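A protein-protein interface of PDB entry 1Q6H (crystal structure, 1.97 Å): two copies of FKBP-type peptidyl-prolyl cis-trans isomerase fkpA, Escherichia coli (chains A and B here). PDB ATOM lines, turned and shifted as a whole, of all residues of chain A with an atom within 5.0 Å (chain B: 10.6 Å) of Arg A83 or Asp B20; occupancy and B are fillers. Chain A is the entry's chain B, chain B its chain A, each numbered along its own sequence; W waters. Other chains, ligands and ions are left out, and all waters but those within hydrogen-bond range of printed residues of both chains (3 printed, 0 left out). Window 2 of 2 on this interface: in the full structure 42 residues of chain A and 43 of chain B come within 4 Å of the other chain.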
ATOM      1  N   ILE A  47      36.578 -20.964   8.761  1.00  0.00           N
ATOM      2  CA  ILE A  47      35.282 -21.519   8.388  1.00  0.00           C
ATOM      3  C   ILE A  47      35.022 -22.779   9.198  1.00  0.00           C
ATOM      4  O   ILE A  47      35.761 -23.729   9.108  1.00  0.00           O
ATOM      5  CB  ILE A  47      35.244 -21.773   6.871  1.00  0.00           C
ATOM      6  CG1 ILE A  47      35.384 -20.428   6.126  1.00  0.00           C
ATOM      7  CG2 ILE A  47      33.956 -22.488   6.453  1.00  0.00           C
ATOM      8  CD1 ILE A  47      35.545 -20.556   4.631  1.00  0.00           C
ATOM      9  N   LYS A  48      33.975 -22.751  10.001  1.00  0.00           N
ATOM     10  CA  LYS A  48      33.654 -23.826  10.910  1.00  0.00           C
ATOM     11  C   LYS A  48      32.245 -24.346  10.595  1.00  0.00           C
ATOM     12  O   LYS A  48      31.249 -23.839  11.089  1.00  0.00           O
ATOM     13  CB  LYS A  48      33.752 -23.334  12.332  1.00  0.00           C
ATOM     14  CG  LYS A  48      35.180 -23.434  12.887  1.00  0.00           C
ATOM     15  CD  LYS A  48      35.362 -22.643  14.163  1.00  0.00           C
ATOM     16  CE  LYS A  48      35.487 -21.144  13.889  1.00  0.00           C
ATOM     17  NZ  LYS A  48      35.600 -20.413  15.176  1.00  0.00           N
ATOM     18  N   LEU A  49      32.180 -25.353   9.739  1.00  0.00           N
ATOM     19  CA  LEU A  49      30.892 -25.900   9.345  1.00  0.00           C
ATOM     20  C   LEU A  49      30.212 -26.635  10.480  1.00  0.00           C
ATOM     21  O   LEU A  49      30.850 -27.133  11.405  1.00  0.00           O
ATOM     22  CB  LEU A  49      31.081 -26.858   8.178  1.00  0.00           C
ATOM     23  CG  LEU A  49      31.339 -26.188   6.836  1.00  0.00           C
ATOM     24  CD1 LEU A  49      31.464 -27.260   5.759  1.00  0.00           C
ATOM     25  CD2 LEU A  49      30.231 -25.229   6.476  1.00  0.00           C
ATOM     26  N   ASP A  50      28.902 -26.722  10.386  1.00  0.00           N
ATOM     27  CA  ASP A  50      28.129 -27.448  11.372  1.00  0.00           C
ATOM     28  C   ASP A  50      28.288 -28.958  11.126  1.00  0.00           C
ATOM     29  O   ASP A  50      27.660 -29.522  10.235  1.00  0.00           O
ATOM     30  CB  ASP A  50      26.673 -27.028  11.258  1.00  0.00           C
ATOM     31  CG  ASP A  50      25.810 -27.670  12.284  1.00  0.00           C
ATOM     32  OD1 ASP A  50      25.992 -28.886  12.541  1.00  0.00           O
ATOM     33  OD2 ASP A  50      24.899 -27.033  12.861  1.00  0.00           O
ATOM     34  N   ALA A  79      28.161 -21.571  -4.100  1.00  0.00           N
ATOM     35  CA  ALA A  79      28.429 -20.420  -3.264  1.00  0.00           C
ATOM     36  C   ALA A  79      29.500 -20.749  -2.223  1.00  0.00           C
ATOM     37  O   ALA A  79      30.419 -19.942  -1.995  1.00  0.00           O
ATOM     38  CB  ALA A  79      27.158 -19.944  -2.599  1.00  0.00           C
ATOM     39  N   PHE A  80      29.397 -21.924  -1.597  1.00  0.00           N
ATOM     40  CA  PHE A  80      30.359 -22.307  -0.566  1.00  0.00           C
ATOM     41  C   PHE A  80      31.785 -22.346  -1.101  1.00  0.00           C
ATOM     42  O   PHE A  80      32.700 -21.797  -0.490  1.00  0.00           O
ATOM     43  CB  PHE A  80      29.994 -23.655   0.052  1.00  0.00           C
ATOM     44  CG  PHE A  80      30.879 -24.017   1.171  1.00  0.00           C
ATOM     45  CD1 PHE A  80      30.848 -23.278   2.350  1.00  0.00           C
ATOM     46  CD2 PHE A  80      31.788 -25.041   1.042  1.00  0.00           C
ATOM     47  CE1 PHE A  80      31.695 -23.576   3.391  1.00  0.00           C
ATOM     48  CE2 PHE A  80      32.633 -25.351   2.081  1.00  0.00           C
ATOM     49  CZ  PHE A  80      32.594 -24.614   3.259  1.00  0.00           C
ATOM     50  N   GLU A  81      31.962 -22.994  -2.246  1.00  0.00           N
ATOM     51  CA  GLU A  81      33.265 -23.157  -2.875  1.00  0.00           C
ATOM     52  C   GLU A  81      33.910 -21.797  -3.251  1.00  0.00           C
ATOM     53  O   GLU A  81      35.144 -21.620  -3.166  1.00  0.00           O
ATOM     54  CB  GLU A  81      33.131 -24.112  -4.078  1.00  0.00           C
ATOM     55  CG  GLU A  81      32.796 -25.554  -3.639  1.00  0.00           C
ATOM     56  CD  GLU A  81      32.034 -26.397  -4.669  1.00  0.00           C
ATOM     57  OE1 GLU A  81      31.407 -25.830  -5.609  1.00  0.00           O
ATOM     58  OE2 GLU A  81      32.039 -27.655  -4.539  1.00  0.00           O
ATOM     59  N   ALA A  82      33.063 -20.843  -3.618  1.00  0.00           N
ATOM     60  CA  ALA A  82      33.477 -19.476  -3.903  1.00  0.00           C
ATOM     61  C   ALA A  82      33.876 -18.742  -2.613  1.00  0.00           C
ATOM     62  O   ALA A  82      34.805 -17.928  -2.603  1.00  0.00           O
ATOM     63  CB  ALA A  82      32.377 -18.739  -4.591  1.00  0.00           C
ATOM     64  N   ARG A  83      33.159 -19.033  -1.537  1.00  0.00           N
ATOM     65  CA  ARG A  83      33.433 -18.431  -0.237  1.00  0.00           C
ATOM     66  C   ARG A  83      34.795 -18.918   0.232  1.00  0.00           C
ATOM     67  O   ARG A  83      35.635 -18.127   0.643  1.00  0.00           O
ATOM     68  CB  ARG A  83      32.339 -18.815   0.765  1.00  0.00           C
ATOM     69  CG  ARG A  83      32.626 -18.450   2.245  1.00  0.00           C
ATOM     70  CD  ARG A  83      31.595 -19.047   3.189  1.00  0.00           C
ATOM     71  NE  ARG A  83      31.904 -18.938   4.613  1.00  0.00           N
ATOM     72  CZ  ARG A  83      31.272 -19.631   5.553  1.00  0.00           C
ATOM     73  NH1 ARG A  83      30.314 -20.490   5.222  1.00  0.00           N
ATOM     74  NH2 ARG A  83      31.582 -19.471   6.832  1.00  0.00           N
ATOM     75  N   VAL A  84      35.018 -20.220   0.111  1.00  0.00           N
ATOM     76  CA  VAL A  84      36.272 -20.847   0.500  1.00  0.00           C
ATOM     77  C   VAL A  84      37.471 -20.329  -0.305  1.00  0.00           C
ATOM     78  O   VAL A  84      38.501 -19.947   0.274  1.00  0.00           O
ATOM     79  CB  VAL A  84      36.191 -22.351   0.340  1.00  0.00           C
ATOM     80  CG1 VAL A  84      37.564 -22.976   0.470  1.00  0.00           C
ATOM     81  CG2 VAL A  84      35.239 -22.929   1.367  1.00  0.00           C
ATOM     82  N   LYS A  85      37.346 -20.339  -1.628  1.00  0.00           N
ATOM     83  CA  LYS A  85      38.424 -19.862  -2.478  1.00  0.00           C
ATOM     84  C   LYS A  85      38.694 -18.393  -2.275  1.00  0.00           C
ATOM     85  O   LYS A  85      39.850 -17.970  -2.309  1.00  0.00           O
ATOM     86  CB  LYS A  85      38.153 -20.181  -3.953  1.00  0.00           C
ATOM     87  CG  LYS A  85      38.284 -21.648  -4.201  1.00  0.00           C
ATOM     88  CD  LYS A  85      38.158 -22.013  -5.644  1.00  0.00           C
ATOM     89  CE  LYS A  85      37.885 -23.504  -5.769  1.00  0.00           C
ATOM     90  NZ  LYS A  85      37.794 -23.930  -7.172  1.00  0.00           N
ATOM     91  N   SER A  86      37.651 -17.618  -2.016  1.00  0.00           N
ATOM     92  CA  SER A  86      37.830 -16.208  -1.779  1.00  0.00           C
ATOM     93  C   SER A  86      38.593 -15.965  -0.480  1.00  0.00           C
ATOM     94  O   SER A  86      39.490 -15.110  -0.392  1.00  0.00           O
ATOM     95  CB  SER A  86      36.498 -15.491  -1.702  1.00  0.00           C
ATOM     96  OG  SER A  86      36.733 -14.240  -1.103  1.00  0.00           O
ATOM     97  N   SER A  87      38.211 -16.704   0.550  1.00  0.00           N
ATOM     98  CA  SER A  87      38.901 -16.620   1.806  1.00  0.00           C
ATOM     99  C   SER A  87      40.349 -17.058   1.656  1.00  0.00           C
ATOM    100  O   SER A  87      41.265 -16.399   2.163  1.00  0.00           O
ATOM    101  CB  SER A  87      38.218 -17.517   2.815  1.00  0.00           C
ATOM    102  OG  SER A  87      37.090 -16.869   3.349  1.00  0.00           O
ATOM    103  N   ALA A  88      40.542 -18.202   1.013  1.00  0.00           N
ATOM    104  CA  ALA A  88      41.869 -18.767   0.826  1.00  0.00           C
ATOM    105  C   ALA A  88      42.765 -17.748   0.135  1.00  0.00           C
ATOM    106  O   ALA A  88      43.886 -17.513   0.556  1.00  0.00           O
ATOM    107  CB  ALA A  88      41.816 -20.053   0.010  1.00  0.00           C
ATOM    108  N   ALA B  15      14.742 -26.135   7.091  1.00  0.00           N
ATOM    109  CA  ALA B  15      14.904 -25.543   8.441  1.00  0.00           C
ATOM    110  C   ALA B  15      16.329 -25.052   8.697  1.00  0.00           C
ATOM    111  O   ALA B  15      16.723 -24.855   9.840  1.00  0.00           O
ATOM    112  CB  ALA B  15      14.483 -26.551   9.500  1.00  0.00           C
ATOM    113  N   PHE B  16      17.098 -24.830   7.634  1.00  0.00           N
ATOM    114  CA  PHE B  16      18.438 -24.288   7.777  1.00  0.00           C
ATOM    115  C   PHE B  16      18.470 -22.799   8.147  1.00  0.00           C
ATOM    116  O   PHE B  16      17.951 -21.928   7.442  1.00  0.00           O
ATOM    117  CB  PHE B  16      19.247 -24.593   6.536  1.00  0.00           C
ATOM    118  CG  PHE B  16      19.268 -26.062   6.220  1.00  0.00           C
ATOM    119  CD1 PHE B  16      19.894 -26.957   7.077  1.00  0.00           C
ATOM    120  CD2 PHE B  16      18.599 -26.556   5.118  1.00  0.00           C
ATOM    121  CE1 PHE B  16      19.877 -28.344   6.800  1.00  0.00           C
ATOM    122  CE2 PHE B  16      18.586 -27.907   4.849  1.00  0.00           C
ATOM    123  CZ  PHE B  16      19.222 -28.799   5.694  1.00  0.00           C
ATOM    124  N   LYS B  17      19.100 -22.537   9.281  1.00  0.00           N
ATOM    125  CA  LYS B  17      19.125 -21.206   9.868  1.00  0.00           C
ATOM    126  C   LYS B  17      20.257 -20.334   9.333  1.00  0.00           C
ATOM    127  O   LYS B  17      20.179 -19.123   9.407  1.00  0.00           O
ATOM    128  CB  LYS B  17      19.272 -21.332  11.383  1.00  0.00           C
ATOM    129  CG  LYS B  17      18.159 -22.093  12.044  1.00  0.00           C
ATOM    130  CD  LYS B  17      16.850 -21.307  12.044  1.00  0.00           C
ATOM    131  CE  LYS B  17      15.703 -22.131  12.628  1.00  0.00           C
ATOM    132  NZ  LYS B  17      15.603 -23.450  11.937  1.00  0.00           N
ATOM    133  N   ASN B  18      21.304 -20.950   8.802  1.00  0.00           N
ATOM    134  CA  ASN B  18      22.450 -20.205   8.312  1.00  0.00           C
ATOM    135  C   ASN B  18      23.317 -21.008   7.366  1.00  0.00           C
ATOM    136  O   ASN B  18      23.135 -22.224   7.216  1.00  0.00           O
ATOM    137  CB  ASN B  18      23.283 -19.697   9.495  1.00  0.00           C
ATOM    138  CG  ASN B  18      23.713 -20.816  10.433  1.00  0.00           C
ATOM    139  OD1 ASN B  18      24.292 -21.796  10.006  1.00  0.00           O
ATOM    140  ND2 ASN B  18      23.448 -20.648  11.729  1.00  0.00           N
ATOM    141  N   ASP B  19      24.267 -20.329   6.733  1.00  0.00           N
ATOM    142  CA  ASP B  19      25.125 -20.977   5.736  1.00  0.00           C
ATOM    143  C   ASP B  19      25.968 -22.115   6.327  1.00  0.00           C
ATOM    144  O   ASP B  19      26.217 -23.120   5.645  1.00  0.00           O
ATOM    145  CB  ASP B  19      26.044 -19.948   5.040  1.00  0.00           C
ATOM    146  CG  ASP B  19      26.737 -20.507   3.790  1.00  0.00           C
ATOM    147  OD1 ASP B  19      26.051 -21.056   2.898  1.00  0.00           O
ATOM    148  OD2 ASP B  19      27.971 -20.386   3.576  1.00  0.00           O
ATOM    149  N   ASP B  20      26.421 -21.960   7.564  1.00  0.00           N
ATOM    150  CA  ASP B  20      27.236 -22.996   8.198  1.00  0.00           C
ATOM    151  C   ASP B  20      26.382 -24.266   8.387  1.00  0.00           C
ATOM    152  O   ASP B  20      26.894 -25.391   8.326  1.00  0.00           O
ATOM    153  CB  ASP B  20      27.847 -22.515   9.512  1.00  0.00           C
ATOM    154  CG  ASP B  20      29.071 -21.571   9.309  1.00  0.00           C
ATOM    155  OD1 ASP B  20      29.676 -21.564   8.222  1.00  0.00           O
ATOM    156  OD2 ASP B  20      29.506 -20.821  10.210  1.00  0.00           O
ATOM    157  N   GLN B  21      25.080 -24.098   8.568  1.00  0.00           N
ATOM    158  CA  GLN B  21      24.217 -25.279   8.614  1.00  0.00           C
ATOM    159  C   GLN B  21      23.940 -25.776   7.182  1.00  0.00           C
ATOM    160  O   GLN B  21      24.090 -26.951   6.901  1.00  0.00           O
ATOM    161  CB  GLN B  21      22.896 -24.991   9.329  1.00  0.00           C
ATOM    162  CG  GLN B  21      23.028 -24.681  10.829  1.00  0.00           C
ATOM    163  CD  GLN B  21      21.666 -24.435  11.490  1.00  0.00           C
ATOM    164  OE1 GLN B  21      20.632 -24.446  10.818  1.00  0.00           O
ATOM    165  NE2 GLN B  21      21.659 -24.242  12.790  1.00  0.00           N
ATOM    166  N   LYS B  22      23.561 -24.861   6.289  1.00  0.00           N
ATOM    167  CA  LYS B  22      23.091 -25.232   4.974  1.00  0.00           C
ATOM    168  C   LYS B  22      24.179 -25.771   4.094  1.00  0.00           C
ATOM    169  O   LYS B  22      24.011 -26.802   3.446  1.00  0.00           O
ATOM    170  CB  LYS B  22      22.410 -24.043   4.294  1.00  0.00           C
ATOM    171  CG  LYS B  22      21.501 -24.448   3.139  1.00  0.00           C
ATOM    172  CD  LYS B  22      20.718 -23.258   2.571  1.00  0.00           C
ATOM    173  CE  LYS B  22      19.894 -23.685   1.372  1.00  0.00           C
ATOM    174  NZ  LYS B  22      19.074 -22.589   0.746  1.00  0.00           N
ATOM    175  N   SER B  23      25.308 -25.077   4.060  1.00  0.00           N
ATOM    176  CA  SER B  23      26.421 -25.531   3.257  1.00  0.00           C
ATOM    177  C   SER B  23      26.935 -26.887   3.780  1.00  0.00           C
ATOM    178  O   SER B  23      27.339 -27.727   3.004  1.00  0.00           O
ATOM    179  CB  SER B  23      27.553 -24.493   3.245  1.00  0.00           C
ATOM    180  OG  SER B  23      27.256 -23.380   2.438  1.00  0.00           O
ATOM    181  N   ALA B  24      26.944 -27.092   5.098  1.00  0.00           N
ATOM    182  CA  ALA B  24      27.453 -28.354   5.642  1.00  0.00           C
ATOM    183  C   ALA B  24      26.522 -29.493   5.163  1.00  0.00           C
ATOM    184  O   ALA B  24      26.985 -30.551   4.704  1.00  0.00           O
ATOM    185  CB  ALA B  24      27.473 -28.304   7.133  1.00  0.00           C
ATOM    186  N   TYR B  25      25.218 -29.241   5.243  1.00  0.00           N
ATOM    187  CA  TYR B  25      24.258 -30.236   4.807  1.00  0.00           C
ATOM    188  C   TYR B  25      24.404 -30.548   3.312  1.00  0.00           C
ATOM    189  O   TYR B  25      24.442 -31.706   2.894  1.00  0.00           O
ATOM    190  CB  TYR B  25      22.854 -29.818   5.151  1.00  0.00           C
ATOM    191  CG  TYR B  25      21.860 -30.902   4.915  1.00  0.00           C
ATOM    192  CD1 TYR B  25      21.264 -31.057   3.668  1.00  0.00           C
ATOM    193  CD2 TYR B  25      21.517 -31.792   5.925  1.00  0.00           C
ATOM    194  CE1 TYR B  25      20.346 -32.058   3.441  1.00  0.00           C
ATOM    195  CE2 TYR B  25      20.627 -32.830   5.691  1.00  0.00           C
ATOM    196  CZ  TYR B  25      20.038 -32.946   4.451  1.00  0.00           C
ATOM    197  OH  TYR B  25      19.121 -33.938   4.191  1.00  0.00           O
ATOM    198  N   ALA B  26      24.521 -29.517   2.500  1.00  0.00           N
ATOM    199  CA  ALA B  26      24.673 -29.715   1.079  1.00  0.00           C
ATOM    200  C   ALA B  26      25.932 -30.528   0.787  1.00  0.00           C
ATOM    201  O   ALA B  26      25.965 -31.396  -0.083  1.00  0.00           O
ATOM    202  CB  ALA B  26      24.738 -28.350   0.368  1.00  0.00           C
ATOM    203  N   LEU B  27      27.006 -30.175   1.466  1.00  0.00           N
ATOM    204  CA  LEU B  27      28.260 -30.881   1.277  1.00  0.00           C
ATOM    205  C   LEU B  27      28.126 -32.379   1.613  1.00  0.00           C
ATOM    206  O   LEU B  27      28.570 -33.272   0.870  1.00  0.00           O
ATOM    207  CB  LEU B  27      29.308 -30.244   2.168  1.00  0.00           C
ATOM    208  CG  LEU B  27      30.594 -30.201   1.386  1.00  0.00           C
ATOM    209  CD1 LEU B  27      31.379 -28.969   1.776  1.00  0.00           C
ATOM    210  CD2 LEU B  27      31.363 -31.478   1.648  1.00  0.00           C
ATOM    211  N   GLY B  28      27.484 -32.649   2.728  1.00  0.00           N
ATOM    212  CA  GLY B  28      27.273 -34.023   3.147  1.00  0.00           C
ATOM    213  C   GLY B  28      26.391 -34.724   2.128  1.00  0.00           C
ATOM    214  O   GLY B  28      26.680 -35.849   1.723  1.00  0.00           O
HETATM  215  O   HOH W   1      32.287 -20.433  10.244  1.00  0.00           O
HETATM  216  O   HOH W   2      28.776 -18.266   8.306  1.00  0.00           O
HETATM  217  O   HOH W   3      26.571 -21.630   0.224  1.00  0.00           O
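Arg A83 touches two residues of chain B.
No residue of chain B comes within 4 Å of Ile A47.
Leu A49 touches just one residue of chain B: Asp B20.
Of the printed residues of chain B, Asp A50 touches Asp B20, Gln B21 and Ala B24.
Ala A79 touches none of the printed residues of chain B.
Phe A80 touches two residues of chain B.
Ala A82 touches none of the printed residues of chain B.
No residue of chain B comes within 4 Å of Ser A86.
Of the printed residues of chain A, Ala B24 touches Asp A50.
Printed residues of chain A within 4 Å of Ser B23: Phe A80.
Printed residues of chain B within 4 Å of Lys A48: Asp B20 (3.6 Å).
Printed residues of chain A within 4 Å of Gln B21: Asp A50 (3.6 Å).
Printed residues of chain A within 4 Å of Asp B19: Arg A83.
Lys A85 touches none of the printed residues of chain B.
The nearest residue of chain A that does not touch Asp B20 is Ile A47 (4.7 Å).
The nearest printed residue of chain A that does not touch Asp B19 is Phe A80 (4.3 Å).
No position is printed for both chains.
Of the 9 pairs that touch across the chains among the printed residues, none has its exchanged pair printed and touching as well.
Water W3 lies within hydrogen-bond range of OD1 of Asp B19 (2.8 Å), OG of Ser B23 (2.9 Å) and N of Phe A80 (3.4 Å).
Water W1 lies within hydrogen-bond range of the side-chain carboxylate of Asp B20 (2.8 Å) and the backbone NH of Lys A48 (2.9 Å).
Water W2 lies within hydrogen-bond range of OD2 of Asp B20 (3.3 Å) and NH2 of Arg A83 (3.4 Å).
Of the 14 printed residues of chain A, 5 touch a printed residue of chain B.
Hydrophobic or aromatic side chains of chain A that line the printed part of chain B: Leu A49 and Phe A80.
Printed residues of chain B that touch a printed residue of chain A: Asp B19, Asp B20, Gln B21, Ser B23, Ala B24 and Leu B27.
Hydrophobic or aromatic side chains of chain B that line the printed part of chain A: Ala B24 and Leu B27.
Among the printed residues, Asp or Glu carboxylates within 4 Å of a Lys or Arg side-chain nitrogen of the other chain: Arg A83 with Asp B19 (2.9 Å) and Arg A83 with Asp B20 (3.2 Å).
The side-chain carboxylate (OD2) of Asp B19 lies within salt-bridge range of the guanidinium group (NH1) of Arg A83, 2.9 Å away.
The backbone NH (N) of Asp A50 is in hydrogen-bond range of the backbone carbonyl oxygen (O) of Asp B20 (3.2 Å).
OD1 of Asp B20 lies within salt-bridge range of NH2 of Arg A83 (3.2 Å).
N of Lys B17 lies within hydrogen-bond range of OE1 of Gln B21, at 2.9 Å.
The side-chain amide oxygen (OD1) of Asn B18 is in hydrogen-bond range of the backbone NH (N) of Asp B20 (3.2 Å).
The side-chain amide oxygen (OD1) of Asn B18 sits at hydrogen-bond distance from the backbone NH (N) of Gln B21, 2.8 Å away.
OG of Ser B23 is in hydrogen-bond range of OD1 of Asp B19 (2.7 Å).
The backbone carbonyl oxygen (O) of Arg A83 lies within hydrogen-bond range of the side-chain hydroxyl (OG) of Ser A87 (3.3 Å).
Among the printed residues, merely in contact across the chains: Asp A50 with Ala B24, Lys A48 with Asp B20, Phe A80 with Ser B23, Asp A50 with Gln B21, Leu A49 with Asp B20 and Phe A80 with Leu B27.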
